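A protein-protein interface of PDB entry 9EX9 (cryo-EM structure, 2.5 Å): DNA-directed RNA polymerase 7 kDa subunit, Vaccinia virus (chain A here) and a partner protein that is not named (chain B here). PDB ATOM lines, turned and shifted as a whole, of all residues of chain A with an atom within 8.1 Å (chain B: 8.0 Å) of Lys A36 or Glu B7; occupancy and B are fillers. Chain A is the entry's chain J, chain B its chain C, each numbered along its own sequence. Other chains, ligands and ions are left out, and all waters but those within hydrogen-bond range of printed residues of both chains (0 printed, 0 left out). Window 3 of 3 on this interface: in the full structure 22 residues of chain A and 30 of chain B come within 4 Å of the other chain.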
ATOM      1  N   CYS A  10      24.769 -31.231  10.934  1.00  0.00           N
ATOM      2  CA  CYS A  10      23.370 -31.579  11.123  1.00  0.00           C
ATOM      3  C   CYS A  10      22.453 -31.053  10.029  1.00  0.00           C
ATOM      4  O   CYS A  10      21.291 -31.464   9.976  1.00  0.00           O
ATOM      5  CB  CYS A  10      22.876 -31.061  12.479  1.00  0.00           C
ATOM      6  SG  CYS A  10      22.779 -29.274  12.606  1.00  0.00           S
ATOM      7  N   LYS A  12      21.273 -27.950   9.561  1.00  0.00           N
ATOM      8  CA  LYS A  12      20.367 -26.877   9.930  1.00  0.00           C
ATOM      9  C   LYS A  12      20.718 -25.584   9.200  1.00  0.00           C
ATOM     10  O   LYS A  12      21.815 -25.415   8.667  1.00  0.00           O
ATOM     11  CB  LYS A  12      20.391 -26.640  11.437  1.00  0.00           C
ATOM     12  CG  LYS A  12      19.401 -27.484  12.203  1.00  0.00           C
ATOM     13  CD  LYS A  12      19.252 -27.012  13.629  1.00  0.00           C
ATOM     14  CE  LYS A  12      18.032 -27.617  14.291  1.00  0.00           C
ATOM     15  NZ  LYS A  12      18.067 -29.098  14.305  1.00  0.00           N
ATOM     16  N   ASP A  13      19.763 -24.659   9.205  1.00  0.00           N
ATOM     17  CA  ASP A  13      19.861 -23.396   8.485  1.00  0.00           C
ATOM     18  C   ASP A  13      20.468 -22.326   9.386  1.00  0.00           C
ATOM     19  O   ASP A  13      19.944 -22.053  10.468  1.00  0.00           O
ATOM     20  CB  ASP A  13      18.466 -22.983   8.013  1.00  0.00           C
ATOM     21  CG  ASP A  13      18.444 -21.650   7.319  1.00  0.00           C
ATOM     22  OD1 ASP A  13      19.516 -21.055   7.114  1.00  0.00           O
ATOM     23  OD2 ASP A  13      17.340 -21.191   6.974  1.00  0.00           O
ATOM     24  N   ILE A  14      21.563 -21.714   8.932  1.00  0.00           N
ATOM     25  CA  ILE A  14      22.289 -20.740   9.743  1.00  0.00           C
ATOM     26  C   ILE A  14      22.537 -19.441   8.988  1.00  0.00           C
ATOM     27  O   ILE A  14      23.457 -18.693   9.324  1.00  0.00           O
ATOM     28  CB  ILE A  14      23.628 -21.323  10.227  1.00  0.00           C
ATOM     29  CG1 ILE A  14      24.506 -21.699   9.035  1.00  0.00           C
ATOM     30  CG2 ILE A  14      23.393 -22.515  11.130  1.00  0.00           C
ATOM     31  CD1 ILE A  14      25.848 -22.244   9.426  1.00  0.00           C
ATOM     32  N   GLU A  17      21.432 -16.076  11.157  1.00  0.00           N
ATOM     33  CA  GLU A  17      22.424 -15.740  12.170  1.00  0.00           C
ATOM     34  C   GLU A  17      23.703 -15.225  11.530  1.00  0.00           C
ATOM     35  O   GLU A  17      24.347 -14.313  12.056  1.00  0.00           O
ATOM     36  CB  GLU A  17      22.711 -16.955  13.049  1.00  0.00           C
ATOM     37  CG  GLU A  17      21.664 -17.213  14.116  1.00  0.00           C
ATOM     38  CD  GLU A  17      20.390 -17.810  13.565  1.00  0.00           C
ATOM     39  OE1 GLU A  17      20.381 -18.217  12.389  1.00  0.00           O
ATOM     40  OE2 GLU A  17      19.393 -17.879  14.310  1.00  0.00           O
ATOM     41  N   VAL A  31      24.119 -13.136  19.025  1.00  0.00           N
ATOM     42  CA  VAL A  31      23.866 -13.973  17.857  1.00  0.00           C
ATOM     43  C   VAL A  31      23.552 -15.399  18.287  1.00  0.00           C
ATOM     44  O   VAL A  31      22.544 -15.981  17.875  1.00  0.00           O
ATOM     45  CB  VAL A  31      25.067 -13.922  16.897  1.00  0.00           C
ATOM     46  CG1 VAL A  31      24.946 -14.988  15.827  1.00  0.00           C
ATOM     47  CG2 VAL A  31      25.167 -12.551  16.272  1.00  0.00           C
ATOM     48  N   LEU A  32      24.396 -15.975  19.141  1.00  0.00           N
ATOM     49  CA  LEU A  32      24.217 -17.366  19.531  1.00  0.00           C
ATOM     50  C   LEU A  32      23.026 -17.580  20.453  1.00  0.00           C
ATOM     51  O   LEU A  32      22.681 -18.735  20.720  1.00  0.00           O
ATOM     52  CB  LEU A  32      25.478 -17.887  20.218  1.00  0.00           C
ATOM     53  CG  LEU A  32      26.736 -18.002  19.367  1.00  0.00           C
ATOM     54  CD1 LEU A  32      27.857 -18.591  20.186  1.00  0.00           C
ATOM     55  CD2 LEU A  32      26.478 -18.843  18.141  1.00  0.00           C
ATOM     56  N   VAL A  33      22.406 -16.516  20.961  1.00  0.00           N
ATOM     57  CA  VAL A  33      21.269 -16.697  21.865  1.00  0.00           C
ATOM     58  C   VAL A  33      20.249 -17.693  21.323  1.00  0.00           C
ATOM     59  O   VAL A  33      19.542 -18.344  22.100  1.00  0.00           O
ATOM     60  CB  VAL A  33      20.601 -15.341  22.160  1.00  0.00           C
ATOM     61  CG1 VAL A  33      19.749 -14.904  20.989  1.00  0.00           C
ATOM     62  CG2 VAL A  33      19.760 -15.437  23.411  1.00  0.00           C
ATOM     63  N   SER A  34      20.139 -17.829  20.001  1.00  0.00           N
ATOM     64  CA  SER A  34      19.102 -18.659  19.395  1.00  0.00           C
ATOM     65  C   SER A  34      19.665 -19.870  18.652  1.00  0.00           C
ATOM     66  O   SER A  34      19.007 -20.392  17.751  1.00  0.00           O
ATOM     67  CB  SER A  34      18.241 -17.825  18.449  1.00  0.00           C
ATOM     68  OG  SER A  34      18.993 -17.370  17.344  1.00  0.00           O
ATOM     69  N   VAL A  35      20.860 -20.326  19.012  1.00  0.00           N
ATOM     70  CA  VAL A  35      21.474 -21.509  18.421  1.00  0.00           C
ATOM     71  C   VAL A  35      21.838 -22.456  19.551  1.00  0.00           C
ATOM     72  O   VAL A  35      22.498 -22.051  20.512  1.00  0.00           O
ATOM     73  CB  VAL A  35      22.717 -21.145  17.592  1.00  0.00           C
ATOM     74  CG1 VAL A  35      23.301 -22.377  16.941  1.00  0.00           C
ATOM     75  CG2 VAL A  35      22.364 -20.115  16.553  1.00  0.00           C
ATOM     76  N   LYS A  36      21.423 -23.713  19.432  1.00  0.00           N
ATOM     77  CA  LYS A  36      21.562 -24.685  20.508  1.00  0.00           C
ATOM     78  C   LYS A  36      22.576 -25.780  20.226  1.00  0.00           C
ATOM     79  O   LYS A  36      23.301 -26.183  21.134  1.00  0.00           O
ATOM     80  CB  LYS A  36      20.207 -25.333  20.802  1.00  0.00           C
ATOM     81  CG  LYS A  36      20.256 -26.418  21.859  1.00  0.00           C
ATOM     82  CD  LYS A  36      18.866 -26.902  22.219  1.00  0.00           C
ATOM     83  CE  LYS A  36      18.916 -27.953  23.313  1.00  0.00           C
ATOM     84  NZ  LYS A  36      17.556 -28.387  23.732  1.00  0.00           N
ATOM     85  N   ASN A  37      22.647 -26.283  19.000  1.00  0.00           N
ATOM     86  CA  ASN A  37      23.503 -27.426  18.725  1.00  0.00           C
ATOM     87  C   ASN A  37      24.971 -27.030  18.738  1.00  0.00           C
ATOM     88  O   ASN A  37      25.348 -25.951  18.282  1.00  0.00           O
ATOM     89  CB  ASN A  37      23.142 -28.047  17.382  1.00  0.00           C
ATOM     90  CG  ASN A  37      21.919 -28.919  17.459  1.00  0.00           C
ATOM     91  OD1 ASN A  37      21.504 -29.328  18.539  1.00  0.00           O
ATOM     92  ND2 ASN A  37      21.337 -29.223  16.310  1.00  0.00           N
ATOM     93  N   GLU A  38      25.800 -27.932  19.256  1.00  0.00           N
ATOM     94  CA  GLU A  38      27.226 -27.664  19.391  1.00  0.00           C
ATOM     95  C   GLU A  38      27.865 -27.371  18.040  1.00  0.00           C
ATOM     96  O   GLU A  38      28.599 -26.387  17.881  1.00  0.00           O
ATOM     97  CB  GLU A  38      27.886 -28.867  20.054  1.00  0.00           C
ATOM     98  CG  GLU A  38      29.359 -28.746  20.300  1.00  0.00           C
ATOM     99  CD  GLU A  38      29.953 -30.052  20.759  1.00  0.00           C
ATOM    100  OE1 GLU A  38      29.627 -31.093  20.156  1.00  0.00           O
ATOM    101  OE2 GLU A  38      30.734 -30.044  21.727  1.00  0.00           O
ATOM    102  N   CYS A  39      27.585 -28.218  17.051  1.00  0.00           N
ATOM    103  CA  CYS A  39      28.166 -28.037  15.728  1.00  0.00           C
ATOM    104  C   CYS A  39      27.833 -26.665  15.161  1.00  0.00           C
ATOM    105  O   CYS A  39      28.701 -25.991  14.597  1.00  0.00           O
ATOM    106  CB  CYS A  39      27.665 -29.138  14.794  1.00  0.00           C
ATOM    107  SG  CYS A  39      25.873 -29.432  14.881  1.00  0.00           S
ATOM    108  N   CYS A  40      26.580 -26.234  15.298  1.00  0.00           N
ATOM    109  CA  CYS A  40      26.172 -24.954  14.733  1.00  0.00           C
ATOM    110  C   CYS A  40      26.891 -23.798  15.410  1.00  0.00           C
ATOM    111  O   CYS A  40      27.307 -22.841  14.746  1.00  0.00           O
ATOM    112  CB  CYS A  40      24.659 -24.798  14.862  1.00  0.00           C
ATOM    113  SG  CYS A  40      23.753 -26.200  14.224  1.00  0.00           S
ATOM    114  N   ARG A  41      27.041 -23.860  16.732  1.00  0.00           N
ATOM    115  CA  ARG A  41      27.764 -22.810  17.436  1.00  0.00           C
ATOM    116  C   ARG A  41      29.208 -22.733  16.964  1.00  0.00           C
ATOM    117  O   ARG A  41      29.727 -21.642  16.698  1.00  0.00           O
ATOM    118  CB  ARG A  41      27.694 -23.055  18.940  1.00  0.00           C
ATOM    119  CG  ARG A  41      26.284 -23.009  19.489  1.00  0.00           C
ATOM    120  CD  ARG A  41      26.203 -23.552  20.894  1.00  0.00           C
ATOM    121  NE  ARG A  41      26.763 -22.637  21.878  1.00  0.00           N
ATOM    122  CZ  ARG A  41      26.098 -21.635  22.433  1.00  0.00           C
ATOM    123  NH1 ARG A  41      24.851 -21.360  22.094  1.00  0.00           N
ATOM    124  NH2 ARG A  41      26.699 -20.889  23.350  1.00  0.00           N
ATOM    125  N   LEU A  44      29.308 -21.145  13.399  1.00  0.00           N
ATOM    126  CA  LEU A  44      29.101 -19.705  13.392  1.00  0.00           C
ATOM    127  C   LEU A  44      30.233 -18.953  14.071  1.00  0.00           C
ATOM    128  O   LEU A  44      30.415 -17.764  13.796  1.00  0.00           O
ATOM    129  CB  LEU A  44      27.775 -19.358  14.060  1.00  0.00           C
ATOM    130  CG  LEU A  44      26.547 -19.514  13.168  1.00  0.00           C
ATOM    131  CD1 LEU A  44      25.290 -19.444  14.000  1.00  0.00           C
ATOM    132  CD2 LEU A  44      26.525 -18.451  12.089  1.00  0.00           C
ATOM    133  N   HIS B   3      12.478 -14.324  16.951  1.00  0.00           N
ATOM    134  CA  HIS B   3      13.467 -14.435  15.896  1.00  0.00           C
ATOM    135  C   HIS B   3      12.827 -14.872  14.588  1.00  0.00           C
ATOM    136  O   HIS B   3      11.738 -15.453  14.579  1.00  0.00           O
ATOM    137  CB  HIS B   3      14.557 -15.439  16.286  1.00  0.00           C
ATOM    138  CG  HIS B   3      15.206 -15.141  17.599  1.00  0.00           C
ATOM    139  ND1 HIS B   3      14.737 -15.646  18.792  1.00  0.00           N
ATOM    140  CD2 HIS B   3      16.283 -14.383  17.910  1.00  0.00           C
ATOM    141  CE1 HIS B   3      15.501 -15.218  19.779  1.00  0.00           C
ATOM    142  NE2 HIS B   3      16.445 -14.448  19.271  1.00  0.00           N
ATOM    143  N   PRO B   4      13.473 -14.595  13.454  1.00  0.00           N
ATOM    144  CA  PRO B   4      12.955 -15.114  12.179  1.00  0.00           C
ATOM    145  C   PRO B   4      12.883 -16.625  12.134  1.00  0.00           C
ATOM    146  O   PRO B   4      12.016 -17.175  11.448  1.00  0.00           O
ATOM    147  CB  PRO B   4      13.954 -14.571  11.149  1.00  0.00           C
ATOM    148  CG  PRO B   4      14.615 -13.431  11.814  1.00  0.00           C
ATOM    149  CD  PRO B   4      14.673 -13.769  13.260  1.00  0.00           C
ATOM    150  N   ARG B   5      13.779 -17.312  12.832  1.00  0.00           N
ATOM    151  CA  ARG B   5      13.835 -18.765  12.844  1.00  0.00           C
ATOM    152  C   ARG B   5      13.922 -19.240  14.285  1.00  0.00           C
ATOM    153  O   ARG B   5      14.705 -18.697  15.068  1.00  0.00           O
ATOM    154  CB  ARG B   5      15.037 -19.264  12.047  1.00  0.00           C
ATOM    155  CG  ARG B   5      15.133 -20.761  11.928  1.00  0.00           C
ATOM    156  CD  ARG B   5      16.517 -21.162  11.499  1.00  0.00           C
ATOM    157  NE  ARG B   5      17.495 -20.897  12.547  1.00  0.00           N
ATOM    158  CZ  ARG B   5      18.163 -21.824  13.221  1.00  0.00           C
ATOM    159  NH1 ARG B   5      18.024 -23.111  12.959  1.00  0.00           N
ATOM    160  NH2 ARG B   5      19.003 -21.446  14.179  1.00  0.00           N
ATOM    161  N   GLU B   6      13.127 -20.250  14.632  1.00  0.00           N
ATOM    162  CA  GLU B   6      13.154 -20.830  15.966  1.00  0.00           C
ATOM    163  C   GLU B   6      13.180 -22.346  15.882  1.00  0.00           C
ATOM    164  O   GLU B   6      12.436 -22.946  15.109  1.00  0.00           O
ATOM    165  CB  GLU B   6      11.955 -20.385  16.785  1.00  0.00           C
ATOM    166  CG  GLU B   6      11.997 -18.930  17.162  1.00  0.00           C
ATOM    167  CD  GLU B   6      11.016 -18.591  18.256  1.00  0.00           C
ATOM    168  OE1 GLU B   6      10.307 -19.510  18.717  1.00  0.00           O
ATOM    169  OE2 GLU B   6      10.953 -17.411  18.656  1.00  0.00           O
ATOM    170  N   GLU B   7      14.027 -22.961  16.698  1.00  0.00           N
ATOM    171  CA  GLU B   7      14.157 -24.409  16.736  1.00  0.00           C
ATOM    172  C   GLU B   7      13.140 -24.987  17.710  1.00  0.00           C
ATOM    173  O   GLU B   7      12.969 -24.462  18.814  1.00  0.00           O
ATOM    174  CB  GLU B   7      15.574 -24.799  17.150  1.00  0.00           C
ATOM    175  CG  GLU B   7      16.667 -24.127  16.340  1.00  0.00           C
ATOM    176  CD  GLU B   7      18.054 -24.485  16.828  1.00  0.00           C
ATOM    177  OE1 GLU B   7      18.177 -24.908  17.993  1.00  0.00           O
ATOM    178  OE2 GLU B   7      19.021 -24.348  16.055  1.00  0.00           O
ATOM    179  N   ASN B   8      12.466 -26.063  17.305  1.00  0.00           N
ATOM    180  CA  ASN B   8      11.435 -26.673  18.133  1.00  0.00           C
ATOM    181  C   ASN B   8      11.493 -28.188  18.014  1.00  0.00           C
ATOM    182  O   ASN B   8      12.089 -28.743  17.087  1.00  0.00           O
ATOM    183  CB  ASN B   8      10.036 -26.188  17.747  1.00  0.00           C
ATOM    184  CG  ASN B   8       9.659 -24.898  18.427  1.00  0.00           C
ATOM    185  OD1 ASN B   8       9.332 -24.882  19.612  1.00  0.00           O
ATOM    186  ND2 ASN B   8       9.688 -23.805  17.680  1.00  0.00           N
ATOM    187  N   SER B   9      10.852 -28.846  18.976  1.00  0.00           N
ATOM    188  CA  SER B   9      10.758 -30.295  19.025  1.00  0.00           C
ATOM    189  C   SER B   9       9.314 -30.703  19.253  1.00  0.00           C
ATOM    190  O   SER B   9       8.574 -30.028  19.971  1.00  0.00           O
ATOM    191  CB  SER B   9      11.624 -30.877  20.138  1.00  0.00           C
ATOM    192  OG  SER B   9      12.977 -30.502  19.978  1.00  0.00           O
ATOM    193  N   PHE B 198      10.551 -35.217  16.607  1.00  0.00           N
ATOM    194  CA  PHE B 198      10.824 -34.428  15.413  1.00  0.00           C
ATOM    195  C   PHE B 198      11.517 -33.140  15.835  1.00  0.00           C
ATOM    196  O   PHE B 198      10.972 -32.385  16.646  1.00  0.00           O
ATOM    197  CB  PHE B 198       9.536 -34.088  14.661  1.00  0.00           C
ATOM    198  CG  PHE B 198       8.717 -35.278  14.265  1.00  0.00           C
ATOM    199  CD1 PHE B 198       7.784 -35.812  15.132  1.00  0.00           C
ATOM    200  CD2 PHE B 198       8.861 -35.845  13.014  1.00  0.00           C
ATOM    201  CE1 PHE B 198       7.025 -36.898  14.764  1.00  0.00           C
ATOM    202  CE2 PHE B 198       8.105 -36.932  12.644  1.00  0.00           C
ATOM    203  CZ  PHE B 198       7.185 -37.456  13.519  1.00  0.00           C
ATOM    204  N   PHE B 199      12.703 -32.890  15.288  1.00  0.00           N
ATOM    205  CA  PHE B 199      13.398 -31.619  15.437  1.00  0.00           C
ATOM    206  C   PHE B 199      13.182 -30.813  14.165  1.00  0.00           C
ATOM    207  O   PHE B 199      13.591 -31.244  13.076  1.00  0.00           O
ATOM    208  CB  PHE B 199      14.890 -31.825  15.689  1.00  0.00           C
ATOM    209  CG  PHE B 199      15.194 -32.637  16.911  1.00  0.00           C
ATOM    210  CD1 PHE B 199      15.046 -32.094  18.172  1.00  0.00           C
ATOM    211  CD2 PHE B 199      15.641 -33.937  16.800  1.00  0.00           C
ATOM    212  CE1 PHE B 199      15.328 -32.834  19.292  1.00  0.00           C
ATOM    213  CE2 PHE B 199      15.925 -34.679  17.921  1.00  0.00           C
ATOM    214  CZ  PHE B 199      15.768 -34.124  19.168  1.00  0.00           C
ATOM    215  N   VAL B 200      12.551 -29.643  14.311  1.00  0.00           N
ATOM    216  CA  VAL B 200      12.063 -28.848  13.190  1.00  0.00           C
ATOM    217  C   VAL B 200      12.393 -27.378  13.424  1.00  0.00           C
ATOM    218  O   VAL B 200      12.777 -26.962  14.520  1.00  0.00           O
ATOM    219  CB  VAL B 200      10.545 -29.019  12.988  1.00  0.00           C
ATOM    220  CG1 VAL B 200      10.178 -30.478  12.956  1.00  0.00           C
ATOM    221  CG2 VAL B 200       9.791 -28.315  14.088  1.00  0.00           C
ATOM    222  N   GLU B 201      12.217 -26.584  12.367  1.00  0.00           N
ATOM    223  CA  GLU B 201      12.482 -25.151  12.380  1.00  0.00           C
ATOM    224  C   GLU B 201      11.226 -24.398  11.971  1.00  0.00           C
ATOM    225  O   GLU B 201      10.607 -24.723  10.955  1.00  0.00           O
ATOM    226  CB  GLU B 201      13.628 -24.800  11.436  1.00  0.00           C
ATOM    227  CG  GLU B 201      14.950 -25.434  11.809  1.00  0.00           C
ATOM    228  CD  GLU B 201      15.985 -25.296  10.718  1.00  0.00           C
ATOM    229  OE1 GLU B 201      15.619 -24.886   9.601  1.00  0.00           O
ATOM    230  OE2 GLU B 201      17.165 -25.599  10.972  1.00  0.00           O
ATOM    231  N   VAL B 202      10.867 -23.386  12.755  1.00  0.00           N
ATOM    232  CA  VAL B 202       9.662 -22.592  12.552  1.00  0.00           C
ATOM    233  C   VAL B 202      10.080 -21.198  12.119  1.00  0.00           C
ATOM    234  O   VAL B 202      10.866 -20.539  12.808  1.00  0.00           O
ATOM    235  CB  VAL B 202       8.814 -22.527  13.834  1.00  0.00           C
ATOM    236  CG1 VAL B 202       7.585 -21.679  13.613  1.00  0.00           C
ATOM    237  CG2 VAL B 202       8.433 -23.917  14.290  1.00  0.00           C
ATOM    238  N   TYR B 203       9.548 -20.747  10.988  1.00  0.00           N
ATOM    239  CA  TYR B 203       9.846 -19.432  10.445  1.00  0.00           C
ATOM    240  C   TYR B 203       8.668 -18.496  10.673  1.00  0.00           C
ATOM    241  O   TYR B 203       7.537 -18.926  10.905  1.00  0.00           O
ATOM    242  CB  TYR B 203      10.177 -19.520   8.955  1.00  0.00           C
ATOM    243  CG  TYR B 203      11.386 -20.371   8.660  1.00  0.00           C
ATOM    244  CD1 TYR B 203      12.663 -19.848   8.741  1.00  0.00           C
ATOM    245  CD2 TYR B 203      11.248 -21.698   8.301  1.00  0.00           C
ATOM    246  CE1 TYR B 203      13.766 -20.623   8.472  1.00  0.00           C
ATOM    247  CE2 TYR B 203      12.346 -22.479   8.030  1.00  0.00           C
ATOM    248  CZ  TYR B 203      13.602 -21.938   8.118  1.00  0.00           C
ATOM    249  OH  TYR B 203      14.697 -22.719   7.850  1.00  0.00           O
ATOM    250  N   LEU B 305       1.869 -26.236  19.665  1.00  0.00           N
ATOM    251  CA  LEU B 305       3.119 -25.483  19.664  1.00  0.00           C
ATOM    252  C   LEU B 305       2.835 -24.003  19.874  1.00  0.00           C
ATOM    253  O   LEU B 305       2.399 -23.312  18.955  1.00  0.00           O
ATOM    254  CB  LEU B 305       3.886 -25.681  18.353  1.00  0.00           C
ATOM    255  CG  LEU B 305       4.656 -26.988  18.159  1.00  0.00           C
ATOM    256  CD1 LEU B 305       5.443 -26.937  16.863  1.00  0.00           C
ATOM    257  CD2 LEU B 305       5.578 -27.266  19.330  1.00  0.00           C
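NH1 of Arg B5 sits close to O of Asp A13 (3.3 Å).
OE2 of Glu A17 lies within salt-bridge range of NH2 of Arg B5 (3.6 Å).
N of Asp A13 is in hydrogen-bond range of OE2 of Glu B201, at 3.3 Å.
OH of Tyr B203 is in hydrogen-bond range of OD2 of Asp A13, at 3.2 Å.
NH2 of Arg B5 lies within salt-bridge range of OE2 of Glu B7 (3.5 Å).
NH1 of Arg B5 is in salt-bridge range of OE2 of Glu B201 (3.3 Å).
The side-chain carboxylate of Glu B201 is in hydrogen-bond range of the side-chain hydroxyl of Tyr B203 (2.9 Å).
The side-chain sulfur (SG) of Cys A10 sits close to the backbone NH (N) of Lys A12 (3.6 Å).
The side-chain hydroxyl (OG) of Ser A34 sits at hydrogen-bond distance from the side-chain carboxylate (OE2) of Glu A17, at 3.1 Å.
Lys A12 touches Glu B7 (CD to OE2, 3.6 Å).
Lys A12 touches Glu B201 (CG to OE2, 3.2 Å).
Val A33 touches His B3.
CB of Ser A34 touches NE2 of His B3, at 3.9 Å.
NH2 of Arg B5 touches O of Ser A34, at 3.7 Å.
Lys A36 touches Glu B7 (CB to OE1, 3.5 Å).
Of chain B, only Glu B7 (3.5 Å) comes within 4 Å of Lys A36.
Glu B7 touches just these residues of chain A: Lys A12 and Lys A36.
No residue of chain A comes within 4 Å of Asn B8.
Printed residues of chain A within 4 Å of Glu B201: Lys A12 (3.2 Å) and Asp A13 (3.3 Å).
Printed residues of chain B within 4 Å of Asp A13: Arg B5, Glu B201 and Tyr B203.
Printed residues of chain A within 4 Å of Tyr B203: Asp A13.
Of the printed residues of chain B, Lys A12 touches Glu B7 and Glu B201.
The nearest residue of chain A that does not touch Glu B7 is Ser A34 (4.3 Å).
Of the 14 printed residues of chain B, 5 touch a printed residue of chain A.
Hydrophobic or aromatic side chains of chain B that line the printed part of chain A: His B3 and Tyr B203.
Of the 17 printed residues of chain A, 6 touch a printed residue of chain B.
Printed residues of chain A that touch a printed residue of chain B: Lys A12, Asp A13, Glu A17, Val A33, Ser A34 and Lys A36.
Hydrophobic or aromatic side chains of chain A within 4 Å of the printed part of chain B: Val A33.
Among the printed residues, Asp or Glu carboxylates within 4 Å of a Lys or Arg side-chain nitrogen of the other chain: Glu A17 with Arg B5 (3.6 Å).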
